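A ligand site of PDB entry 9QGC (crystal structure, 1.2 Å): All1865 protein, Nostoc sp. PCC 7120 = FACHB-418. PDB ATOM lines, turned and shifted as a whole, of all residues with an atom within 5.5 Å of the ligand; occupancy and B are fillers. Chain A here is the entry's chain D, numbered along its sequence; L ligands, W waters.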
ATOM      1  N   ALA A  35     -11.485   8.674 -12.370  1.00  0.00           N
ATOM      2  CA  ALA A  35     -11.196   9.770 -11.444  1.00  0.00           C
ATOM      3  C   ALA A  35      -9.847   9.537 -10.771  1.00  0.00           C
ATOM      4  O   ALA A  35      -9.381   8.385 -10.663  1.00  0.00           O
ATOM      5  CB  ALA A  35     -12.247   9.758 -10.334  1.00  0.00           C
ATOM      6  N   PRO A  36      -9.193  10.603 -10.280  1.00  0.00           N
ATOM      7  CA  PRO A  36      -7.948  10.455  -9.563  1.00  0.00           C
ATOM      8  C   PRO A  36      -8.142   9.700  -8.249  1.00  0.00           C
ATOM      9  O   PRO A  36      -9.045   9.995  -7.486  1.00  0.00           O
ATOM     10  CB  PRO A  36      -7.439  11.890  -9.338  1.00  0.00           C
ATOM     11  CG  PRO A  36      -8.736  12.702  -9.355  1.00  0.00           C
ATOM     12  CD  PRO A  36      -9.672  11.990 -10.359  1.00  0.00           C
ATOM     13  N   LEU A  37      -7.281   8.688  -8.004  1.00  0.00           N
ATOM     14  CA  LEU A  37      -7.438   7.835  -6.824  1.00  0.00           C
ATOM     15  C   LEU A  37      -6.075   7.544  -6.203  1.00  0.00           C
ATOM     16  O   LEU A  37      -5.272   6.756  -6.754  1.00  0.00           O
ATOM     17  CB  LEU A  37      -8.078   6.501  -7.259  1.00  0.00           C
ATOM     18  CG  LEU A  37      -9.499   6.604  -7.829  1.00  0.00           C
ATOM     19  CD1 LEU A  37      -9.788   5.410  -8.737  1.00  0.00           C
ATOM     20  CD2 LEU A  37     -10.558   6.730  -6.727  1.00  0.00           C
ATOM     21  N   THR A  38      -5.832   8.190  -5.057  1.00  0.00           N
ATOM     22  CA  THR A  38      -4.683   7.889  -4.222  1.00  0.00           C
ATOM     23  C   THR A  38      -4.686   6.406  -3.811  1.00  0.00           C
ATOM     24  O   THR A  38      -5.648   5.972  -3.203  1.00  0.00           O
ATOM     25  CB  THR A  38      -4.737   8.823  -2.996  1.00  0.00           C
ATOM     26  OG1 THR A  38      -4.506  10.168  -3.391  1.00  0.00           O
ATOM     27  CG2 THR A  38      -3.707   8.459  -1.925  1.00  0.00           C
ATOM     28  N   ARG A  39      -3.624   5.706  -4.170  1.00  0.00           N
ATOM     29  CA  ARG A  39      -3.472   4.288  -3.819  1.00  0.00           C
ATOM     30  C   ARG A  39      -2.282   4.040  -2.917  1.00  0.00           C
ATOM     31  O   ARG A  39      -2.111   2.899  -2.449  1.00  0.00           O
ATOM     32  CB  ARG A  39      -3.421   3.430  -5.073  1.00  0.00           C
ATOM     33  CG  ARG A  39      -4.568   3.662  -6.063  1.00  0.00           C
ATOM     34  CD  ARG A  39      -6.000   3.517  -5.516  1.00  0.00           C
ATOM     35  NE  ARG A  39      -6.154   2.200  -4.849  1.00  0.00           N
ATOM     36  CZ  ARG A  39      -6.495   1.093  -5.505  1.00  0.00           C
ATOM     37  NH1 ARG A  39      -6.684   1.102  -6.825  1.00  0.00           N
ATOM     38  NH2 ARG A  39      -6.528  -0.100  -4.868  1.00  0.00           N
ATOM     39  N   GLU A  68      -3.665   9.505  -9.977  1.00  0.00           N
ATOM     40  CA  GLU A  68      -3.760   9.856  -8.560  1.00  0.00           C
ATOM     41  C   GLU A  68      -3.042  11.170  -8.264  1.00  0.00           C
ATOM     42  O   GLU A  68      -2.035  11.531  -8.894  1.00  0.00           O
ATOM     43  CB  GLU A  68      -3.066   8.746  -7.757  1.00  0.00           C
ATOM     44  CG  GLU A  68      -1.545   8.588  -7.964  1.00  0.00           C
ATOM     45  CD  GLU A  68      -1.024   7.190  -7.738  1.00  0.00           C
ATOM     46  OE1 GLU A  68      -0.793   6.840  -6.583  1.00  0.00           O
ATOM     47  OE2 GLU A  68      -0.897   6.422  -8.755  1.00  0.00           O
ATOM     48  N   ALA A  69      -3.530  11.839  -7.182  1.00  0.00           N
ATOM     49  CA  ALA A  69      -2.853  13.048  -6.729  1.00  0.00           C
ATOM     50  C   ALA A  69      -1.356  12.776  -6.520  1.00  0.00           C
ATOM     51  O   ALA A  69      -0.938  11.820  -5.838  1.00  0.00           O
ATOM     52  CB  ALA A  69      -3.527  13.508  -5.440  1.00  0.00           C
ATOM     53  N   GLN A 111      -2.708  14.296 -11.944  1.00  0.00           N
ATOM     54  CA  GLN A 111      -3.268  15.293 -11.027  1.00  0.00           C
ATOM     55  C   GLN A 111      -2.155  15.851 -10.144  1.00  0.00           C
ATOM     56  O   GLN A 111      -1.450  15.093  -9.447  1.00  0.00           O
ATOM     57  CB  GLN A 111      -4.355  14.655 -10.160  1.00  0.00           C
ATOM     58  CG  GLN A 111      -5.105  15.734  -9.387  1.00  0.00           C
ATOM     59  CD  GLN A 111      -6.088  15.191  -8.383  1.00  0.00           C
ATOM     60  OE1 GLN A 111      -5.708  14.391  -7.511  1.00  0.00           O
ATOM     61  NE2 GLN A 111      -7.311  15.715  -8.434  1.00  0.00           N
ATOM     62  N   GLU A 185      -4.081  17.822 -14.353  1.00  0.00           N
ATOM     63  CA  GLU A 185      -5.263  18.337 -13.634  1.00  0.00           C
ATOM     64  C   GLU A 185      -4.744  19.016 -12.368  1.00  0.00           C
ATOM     65  O   GLU A 185      -3.981  18.416 -11.603  1.00  0.00           O
ATOM     66  CB  GLU A 185      -6.255  17.206 -13.307  1.00  0.00           C
ATOM     67  CG  GLU A 185      -7.455  17.731 -12.520  1.00  0.00           C
ATOM     68  CD  GLU A 185      -8.481  16.660 -12.210  1.00  0.00           C
ATOM     69  OE1 GLU A 185      -8.425  16.080 -11.077  1.00  0.00           O
ATOM     70  OE2 GLU A 185      -9.289  16.314 -13.127  1.00  0.00           O
ATOM     71  N   HIS A 187      -5.221  19.927  -8.697  1.00  0.00           N
ATOM     72  CA  HIS A 187      -6.083  19.507  -7.598  1.00  0.00           C
ATOM     73  C   HIS A 187      -6.450  20.698  -6.700  1.00  0.00           C
ATOM     74  O   HIS A 187      -5.648  21.109  -5.855  1.00  0.00           O
ATOM     75  CB  HIS A 187      -5.386  18.429  -6.765  1.00  0.00           C
ATOM     76  CG  HIS A 187      -6.330  17.743  -5.828  1.00  0.00           C
ATOM     77  ND1 HIS A 187      -6.111  16.557  -5.136  1.00  0.00           N
ATOM     78  CD2 HIS A 187      -7.564  18.149  -5.490  1.00  0.00           C
ATOM     79  CE1 HIS A 187      -7.208  16.244  -4.447  1.00  0.00           C
ATOM     80  NE2 HIS A 187      -8.100  17.211  -4.687  1.00  0.00           N
ATOM     81  N   ALA A 189      -9.291  20.792  -4.930  1.00  0.00           N
ATOM     82  CA  ALA A 189     -10.426  20.197  -4.242  1.00  0.00           C
ATOM     83  C   ALA A 189      -9.998  19.559  -2.911  1.00  0.00           C
ATOM     84  O   ALA A 189      -8.811  19.603  -2.530  1.00  0.00           O
ATOM     85  CB  ALA A 189     -11.097  19.165  -5.144  1.00  0.00           C
ATOM     86  N   ASN A 190     -10.993  18.965  -2.232  1.00  0.00           N
ATOM     87  CA  ASN A 190     -10.854  18.073  -1.090  1.00  0.00           C
ATOM     88  C   ASN A 190     -10.044  18.689   0.050  1.00  0.00           C
ATOM     89  O   ASN A 190      -9.491  17.945   0.873  1.00  0.00           O
ATOM     90  CB  ASN A 190     -10.325  16.712  -1.524  1.00  0.00           C
ATOM     91  CG  ASN A 190     -11.300  16.040  -2.476  1.00  0.00           C
ATOM     92  OD1 ASN A 190     -12.480  16.448  -2.552  1.00  0.00           O
ATOM     93  ND2 ASN A 190     -10.839  15.036  -3.203  1.00  0.00           N
ATOM     94  N   ARG A 239      -9.801  20.693 -10.833  1.00  0.00           N
ATOM     95  CA  ARG A 239     -10.833  19.970 -10.070  1.00  0.00           C
ATOM     96  C   ARG A 239     -11.235  20.801  -8.850  1.00  0.00           C
ATOM     97  O   ARG A 239     -10.369  21.304  -8.115  1.00  0.00           O
ATOM     98  CB  ARG A 239     -10.294  18.609  -9.626  1.00  0.00           C
ATOM     99  CG  ARG A 239     -11.468  17.718  -9.185  1.00  0.00           C
ATOM    100  CD  ARG A 239     -10.988  16.314  -8.819  1.00  0.00           C
ATOM    101  NE  ARG A 239     -12.144  15.393  -8.976  1.00  0.00           N
ATOM    102  CZ  ARG A 239     -12.290  14.185  -8.416  1.00  0.00           C
ATOM    103  NH1 ARG A 239     -11.562  13.826  -7.362  1.00  0.00           N
ATOM    104  NH2 ARG A 239     -13.247  13.363  -8.854  1.00  0.00           N
ATOM    105  N   PHE A 276     -16.249  17.334  -8.352  1.00  0.00           N
ATOM    106  CA  PHE A 276     -16.599  16.239  -7.439  1.00  0.00           C
ATOM    107  C   PHE A 276     -17.807  16.683  -6.618  1.00  0.00           C
ATOM    108  O   PHE A 276     -17.673  17.633  -5.833  1.00  0.00           O
ATOM    109  CB  PHE A 276     -15.382  15.926  -6.568  1.00  0.00           C
ATOM    110  CG  PHE A 276     -15.617  14.989  -5.389  1.00  0.00           C
ATOM    111  CD1 PHE A 276     -16.705  14.128  -5.330  1.00  0.00           C
ATOM    112  CD2 PHE A 276     -14.681  14.964  -4.361  1.00  0.00           C
ATOM    113  CE1 PHE A 276     -16.874  13.273  -4.235  1.00  0.00           C
ATOM    114  CE2 PHE A 276     -14.818  14.109  -3.284  1.00  0.00           C
ATOM    115  CZ  PHE A 276     -15.929  13.268  -3.207  1.00  0.00           C
ATOM    116  N   ILE A 279     -21.046  13.254  -1.942  1.00  0.00           N
ATOM    117  CA  ILE A 279     -22.067  12.205  -1.871  1.00  0.00           C
ATOM    118  C   ILE A 279     -23.144  12.577  -0.835  1.00  0.00           C
ATOM    119  O   ILE A 279     -24.292  12.176  -0.960  1.00  0.00           O
ATOM    120  CB  ILE A 279     -21.370  10.846  -1.530  1.00  0.00           C
ATOM    121  CG1 ILE A 279     -20.444  10.384  -2.658  1.00  0.00           C
ATOM    122  CG2 ILE A 279     -22.267   9.732  -1.000  1.00  0.00           C
ATOM    123  CD1 ILE A 279     -20.998  10.668  -4.031  1.00  0.00           C
ATOM    124  N   ASN A 306     -18.714  14.046 -11.215  1.00  0.00           N
ATOM    125  CA  ASN A 306     -18.268  12.860 -10.499  1.00  0.00           C
ATOM    126  C   ASN A 306     -19.000  12.794  -9.164  1.00  0.00           C
ATOM    127  O   ASN A 306     -19.320  13.823  -8.552  1.00  0.00           O
ATOM    128  CB  ASN A 306     -16.758  12.979 -10.254  1.00  0.00           C
ATOM    129  CG  ASN A 306     -16.272  12.084  -9.153  1.00  0.00           C
ATOM    130  OD1 ASN A 306     -16.225  12.528  -7.999  1.00  0.00           O
ATOM    131  ND2 ASN A 306     -16.016  10.826  -9.459  1.00  0.00           N
ATOM    132  N   GLY A 307     -19.180  11.564  -8.650  1.00  0.00           N
ATOM    133  CA  GLY A 307     -19.666  11.352  -7.289  1.00  0.00           C
ATOM    134  C   GLY A 307     -20.875  10.422  -7.346  1.00  0.00           C
ATOM    135  O   GLY A 307     -21.988  10.880  -7.591  1.00  0.00           O
ATOM    136  N   GLY A 308     -20.653   9.116  -7.128  1.00  0.00           N
ATOM    137  CA  GLY A 308     -21.785   8.196  -7.069  1.00  0.00           C
ATOM    138  C   GLY A 308     -22.441   7.886  -8.415  1.00  0.00           C
ATOM    139  O   GLY A 308     -23.581   7.410  -8.443  1.00  0.00           O
ATOM    140  N   TYR A 309     -21.767   8.162  -9.558  1.00  0.00           N
ATOM    141  CA  TYR A 309     -22.411   7.914 -10.854  1.00  0.00           C
ATOM    142  C   TYR A 309     -22.556   6.420 -11.146  1.00  0.00           C
ATOM    143  O   TYR A 309     -21.786   5.568 -10.682  1.00  0.00           O
ATOM    144  CB  TYR A 309     -21.706   8.676 -11.981  1.00  0.00           C
ATOM    145  CG  TYR A 309     -22.164  10.114 -11.968  1.00  0.00           C
ATOM    146  CD1 TYR A 309     -21.595  11.056 -11.100  1.00  0.00           C
ATOM    147  CD2 TYR A 309     -23.219  10.548 -12.780  1.00  0.00           C
ATOM    148  CE1 TYR A 309     -22.077  12.355 -11.016  1.00  0.00           C
ATOM    149  CE2 TYR A 309     -23.698  11.837 -12.716  1.00  0.00           C
ATOM    150  CZ  TYR A 309     -23.130  12.730 -11.839  1.00  0.00           C
ATOM    151  OH  TYR A 309     -23.595  14.002 -11.776  1.00  0.00           O
ATOM    152  N   ALA A 327     -16.733  11.086 -14.501  1.00  0.00           N
ATOM    153  CA  ALA A 327     -15.644  10.354 -13.866  1.00  0.00           C
ATOM    154  C   ALA A 327     -16.149   9.401 -12.784  1.00  0.00           C
ATOM    155  O   ALA A 327     -17.027   9.746 -11.984  1.00  0.00           O
ATOM    156  CB  ALA A 327     -14.599  11.323 -13.297  1.00  0.00           C
ATOM    157  N   PHE A 328     -15.544   8.209 -12.781  1.00  0.00           N
ATOM    158  CA  PHE A 328     -15.862   7.176 -11.796  1.00  0.00           C
ATOM    159  C   PHE A 328     -14.597   6.898 -10.998  1.00  0.00           C
ATOM    160  O   PHE A 328     -13.512   6.706 -11.587  1.00  0.00           O
ATOM    161  CB  PHE A 328     -16.289   5.880 -12.515  1.00  0.00           C
ATOM    162  CG  PHE A 328     -17.571   6.052 -13.313  1.00  0.00           C
ATOM    163  CD1 PHE A 328     -17.540   6.580 -14.608  1.00  0.00           C
ATOM    164  CD2 PHE A 328     -18.795   5.631 -12.781  1.00  0.00           C
ATOM    165  CE1 PHE A 328     -18.719   6.729 -15.361  1.00  0.00           C
ATOM    166  CE2 PHE A 328     -19.960   5.740 -13.553  1.00  0.00           C
ATOM    167  CZ  PHE A 328     -19.919   6.282 -14.835  1.00  0.00           C
ATOM    168  N   GLY A 329     -14.736   6.899  -9.674  1.00  0.00           N
ATOM    169  CA  GLY A 329     -13.601   6.554  -8.804  1.00  0.00           C
ATOM    170  C   GLY A 329     -13.702   5.113  -8.337  1.00  0.00           C
ATOM    171  O   GLY A 329     -13.007   4.251  -8.860  1.00  0.00           O
ATOM    172  N   THR A 330     -14.560   4.882  -7.340  1.00  0.00           N
ATOM    173  CA  THR A 330     -14.628   3.576  -6.666  1.00  0.00           C
ATOM    174  C   THR A 330     -14.808   2.446  -7.701  1.00  0.00           C
ATOM    175  O   THR A 330     -14.143   1.421  -7.619  1.00  0.00           O
ATOM    176  CB  THR A 330     -15.853   3.626  -5.734  1.00  0.00           C
ATOM    177  OG1 THR A 330     -15.662   4.686  -4.794  1.00  0.00           O
ATOM    178  CG2 THR A 330     -15.953   2.335  -4.966  1.00  0.00           C
ATOM    179  N   LEU A 331     -15.664   2.621  -8.705  1.00  0.00           N
ATOM    180  CA  LEU A 331     -15.924   1.528  -9.640  1.00  0.00           C
ATOM    181  C   LEU A 331     -14.692   1.221 -10.486  1.00  0.00           C
ATOM    182  O   LEU A 331     -14.553   0.080 -10.918  1.00  0.00           O
ATOM    183  CB  LEU A 331     -17.126   1.820 -10.544  1.00  0.00           C
ATOM    184  CG  LEU A 331     -18.499   1.640  -9.917  1.00  0.00           C
ATOM    185  CD1 LEU A 331     -19.587   2.105 -10.876  1.00  0.00           C
ATOM    186  CD2 LEU A 331     -18.741   0.198  -9.440  1.00  0.00           C
ATOM    187  N   ILE A 333     -11.635   1.345  -9.265  1.00  0.00           N
ATOM    188  CA  ILE A 333     -10.740   0.555  -8.432  1.00  0.00           C
ATOM    189  C   ILE A 333     -10.991  -0.920  -8.747  1.00  0.00           C
ATOM    190  O   ILE A 333     -10.056  -1.685  -9.010  1.00  0.00           O
ATOM    191  CB  ILE A 333     -10.935   0.885  -6.948  1.00  0.00           C
ATOM    192  CG1 ILE A 333     -10.524   2.337  -6.639  1.00  0.00           C
ATOM    193  CG2 ILE A 333     -10.198  -0.135  -6.060  1.00  0.00           C
ATOM    194  CD1 ILE A 333     -10.784   2.736  -5.189  1.00  0.00           C
ATOM    195  N   PHE A 356      -7.573  -0.238  -0.457  1.00  0.00           N
ATOM    196  CA  PHE A 356      -7.461   0.979  -1.229  1.00  0.00           C
ATOM    197  C   PHE A 356      -6.054   1.568  -1.145  1.00  0.00           C
ATOM    198  O   PHE A 356      -5.542   2.084  -2.153  1.00  0.00           O
ATOM    199  CB  PHE A 356      -8.494   2.048  -0.822  1.00  0.00           C
ATOM    200  CG  PHE A 356      -9.930   1.749  -1.223  1.00  0.00           C
ATOM    201  CD1 PHE A 356     -10.257   0.663  -2.057  1.00  0.00           C
ATOM    202  CD2 PHE A 356     -10.950   2.636  -0.822  1.00  0.00           C
ATOM    203  CE1 PHE A 356     -11.587   0.423  -2.439  1.00  0.00           C
ATOM    204  CE2 PHE A 356     -12.275   2.395  -1.212  1.00  0.00           C
ATOM    205  CZ  PHE A 356     -12.595   1.284  -2.003  1.00  0.00           C
ATOM    206  N   TYR A 357      -5.465   1.570   0.067  1.00  0.00           N
ATOM    207  CA  TYR A 357      -4.237   2.297   0.318  1.00  0.00           C
ATOM    208  C   TYR A 357      -3.126   1.348   0.722  1.00  0.00           C
ATOM    209  O   TYR A 357      -3.287   0.574   1.658  1.00  0.00           O
ATOM    210  CB  TYR A 357      -4.481   3.330   1.432  1.00  0.00           C
ATOM    211  CG  TYR A 357      -5.576   4.332   1.128  1.00  0.00           C
ATOM    212  CD1 TYR A 357      -5.396   5.300   0.154  1.00  0.00           C
ATOM    213  CD2 TYR A 357      -6.783   4.324   1.830  1.00  0.00           C
ATOM    214  CE1 TYR A 357      -6.369   6.237  -0.133  1.00  0.00           C
ATOM    215  CE2 TYR A 357      -7.756   5.284   1.562  1.00  0.00           C
ATOM    216  CZ  TYR A 357      -7.551   6.256   0.587  1.00  0.00           C
ATOM    217  OH  TYR A 357      -8.485   7.257   0.342  1.00  0.00           O
HETATM  218  N1  LIG L   1      -9.848  12.679  -5.339  1.00  0.00           N
HETATM  219  C1  LIG L   1      -8.860  13.416  -5.844  1.00  0.00           C
HETATM  220  O1  LIG L   1      -9.064  14.534  -6.359  1.00  0.00           O
HETATM  221  N2  LIG L   1      -7.537  12.968  -5.882  1.00  0.00           N
HETATM  222  C2  LIG L   1      -7.178  11.781  -5.277  1.00  0.00           C
HETATM  223  O2  LIG L   1      -6.008  11.386  -5.412  1.00  0.00           O
HETATM  224  C3  LIG L   1      -8.211  10.987  -4.693  1.00  0.00           C
HETATM  225  N3  LIG L   1      -7.899   9.835  -4.084  1.00  0.00           N
HETATM  226  C4  LIG L   1      -8.936   9.018  -3.714  1.00  0.00           C
HETATM  227  C5  LIG L   1      -8.644   7.733  -3.226  1.00  0.00           C
HETATM  228  C6  LIG L   1      -9.641   6.839  -2.900  1.00  0.00           C
HETATM  229  C7  LIG L   1      -9.279   5.455  -2.439  1.00  0.00           C
HETATM  230  C8  LIG L   1     -10.998   7.223  -3.084  1.00  0.00           C
HETATM  231  C9  LIG L   1     -12.119   6.226  -2.812  1.00  0.00           C
HETATM  232  C10 LIG L   1     -11.283   8.513  -3.523  1.00  0.00           C
HETATM  233  C11 LIG L   1     -10.276   9.417  -3.868  1.00  0.00           C
HETATM  234  N4  LIG L   1     -10.554  10.691  -4.369  1.00  0.00           N
HETATM  235  C12 LIG L   1      -9.537  11.511  -4.808  1.00  0.00           C
HETATM  236  C13 LIG L   1     -11.940  11.073  -4.669  1.00  0.00           C
HETATM  237  C14 LIG L   1     -12.386  10.323  -5.964  1.00  0.00           C
HETATM  238  O3  LIG L   1     -11.675  10.867  -7.105  1.00  0.00           O
HETATM  239  C15 LIG L   1     -13.865  10.536  -6.279  1.00  0.00           C
HETATM  240  O4  LIG L   1     -14.082  11.944  -6.491  1.00  0.00           O
HETATM  241  C16 LIG L   1     -14.815  10.049  -5.189  1.00  0.00           C
HETATM  242  O5  LIG L   1     -14.426   8.724  -4.804  1.00  0.00           O
HETATM  243  C17 LIG L   1     -16.255  10.063  -5.628  1.00  0.00           C
HETATM  244  O6  LIG L   1     -16.462   9.370  -6.883  1.00  0.00           O
HETATM  245  P1  LIG L   1     -17.020   7.851  -6.901  1.00  0.00           P
HETATM  246  O7  LIG L   1     -17.117   7.540  -8.388  1.00  0.00           O
HETATM  247  O8  LIG L   1     -18.334   7.866  -6.189  1.00  0.00           O
HETATM  248  O9  LIG L   1     -15.990   6.970  -6.188  1.00  0.00           O
HETATM  249  O   HOH W   1     -18.814   8.994  -9.915  1.00  0.00           O
HETATM  250  O   HOH W   2     -14.908   8.916  -2.134  1.00  0.00           O
HETATM  251  O   HOH W   3     -19.795   5.572  -6.107  1.00  0.00           O
HETATM  252  O   HOH W   4     -18.520   7.805  -3.483  1.00  0.00           O
HETATM  253  O   HOH W   5     -17.505   4.868  -9.149  1.00  0.00           O
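The side-chain amide oxygen (OD1) of Asn 306 is in hydrogen-bond range of an oxygen (O4) of the ligand (2.7 Å). O9 of the ligand sits at hydrogen-bond distance from N of Thr 330, 2.8 Å away. An oxygen (O9) of the ligand is in hydrogen-bond range of the side-chain hydroxyl of Thr 330 (2.7 Å). The backbone NH (N) of Gly 329 lies within hydrogen-bond range of an oxygen (O7) of the ligand, at 2.8 Å. The guanidinium group (NH1) of Arg 239 sits at hydrogen-bond distance from an oxygen (O1) of the ligand (2.8 Å). N of Thr 38 sits at hydrogen-bond distance from N3 of the ligand (2.8 Å). OG1 of Thr 38 sits at hydrogen-bond distance from O2 of the ligand (2.8 Å). The backbone NH (N) of Gly 308 sits at hydrogen-bond distance from an oxygen (O8) of the ligand (2.8 Å). An oxygen (O3) of the ligand sits at hydrogen-bond distance from the backbone carbonyl oxygen (O) of Pro 36 (2.8 Å). The side-chain amide oxygen (OE1) of Gln 111 sits at hydrogen-bond distance from a nitrogen (N2) of the ligand (2.8 Å). O2 of the ligand sits at hydrogen-bond distance from N of Ala 69, 3.1 Å away. An oxygen (O1) of the ligand lies close to a ring nitrogen (NE2) of His 187 (3.3 Å). The side-chain amide nitrogen of Asn 190 sits at hydrogen-bond distance from a nitrogen (N1) of the ligand, at 3.3 Å.
NH2 of Arg 239 is in hydrogen-bond range of OD1 of Asn 306 (3.2 Å). The side-chain amide nitrogen of Asn 306 is in hydrogen-bond range of the backbone carbonyl oxygen of Ala 327. O of Arg 239 is in hydrogen-bond range of N of Ala 189 (3.4 Å). The side-chain amide oxygen (OE1) of Gln 111 lies close to the backbone NH (N) of Ala 69 (3.4 Å). The side-chain amide oxygen (OE1) of Gln 111 sits at hydrogen-bond distance from a ring nitrogen (ND1) of His 187 (3.2 Å). NE2 of Gln 111 is in hydrogen-bond range of OE1 of Glu 185 (2.9 Å). NE2 of His 187 lies within hydrogen-bond range of O of Ala 189 (3.3 Å). N of Ala 35 lies within hydrogen-bond range of O of Phe 328, at 2.9 Å.
Ala 35 touches the ligand (CB to O3, 3.5 Å). CA of Leu 37 touches N3 of the ligand, 3.4 Å away. Phe 276 touches the ligand (CE1 to C17, 3.6 Å). Gly 307 touches the ligand. Phe 328 touches the ligand. Phe 356 touches the ligand (CD2 to C7, 3.7 Å). Tyr 357 touches the ligand. Hydrophobic or aromatic side chains within 4 Å of the ligand: Ala 35, Pro 36, Leu 37, Ala 69, His 187, Phe 276, Phe 356 and Tyr 357. Of the 27 residues printed, 18 come within 4 Å of the ligand.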
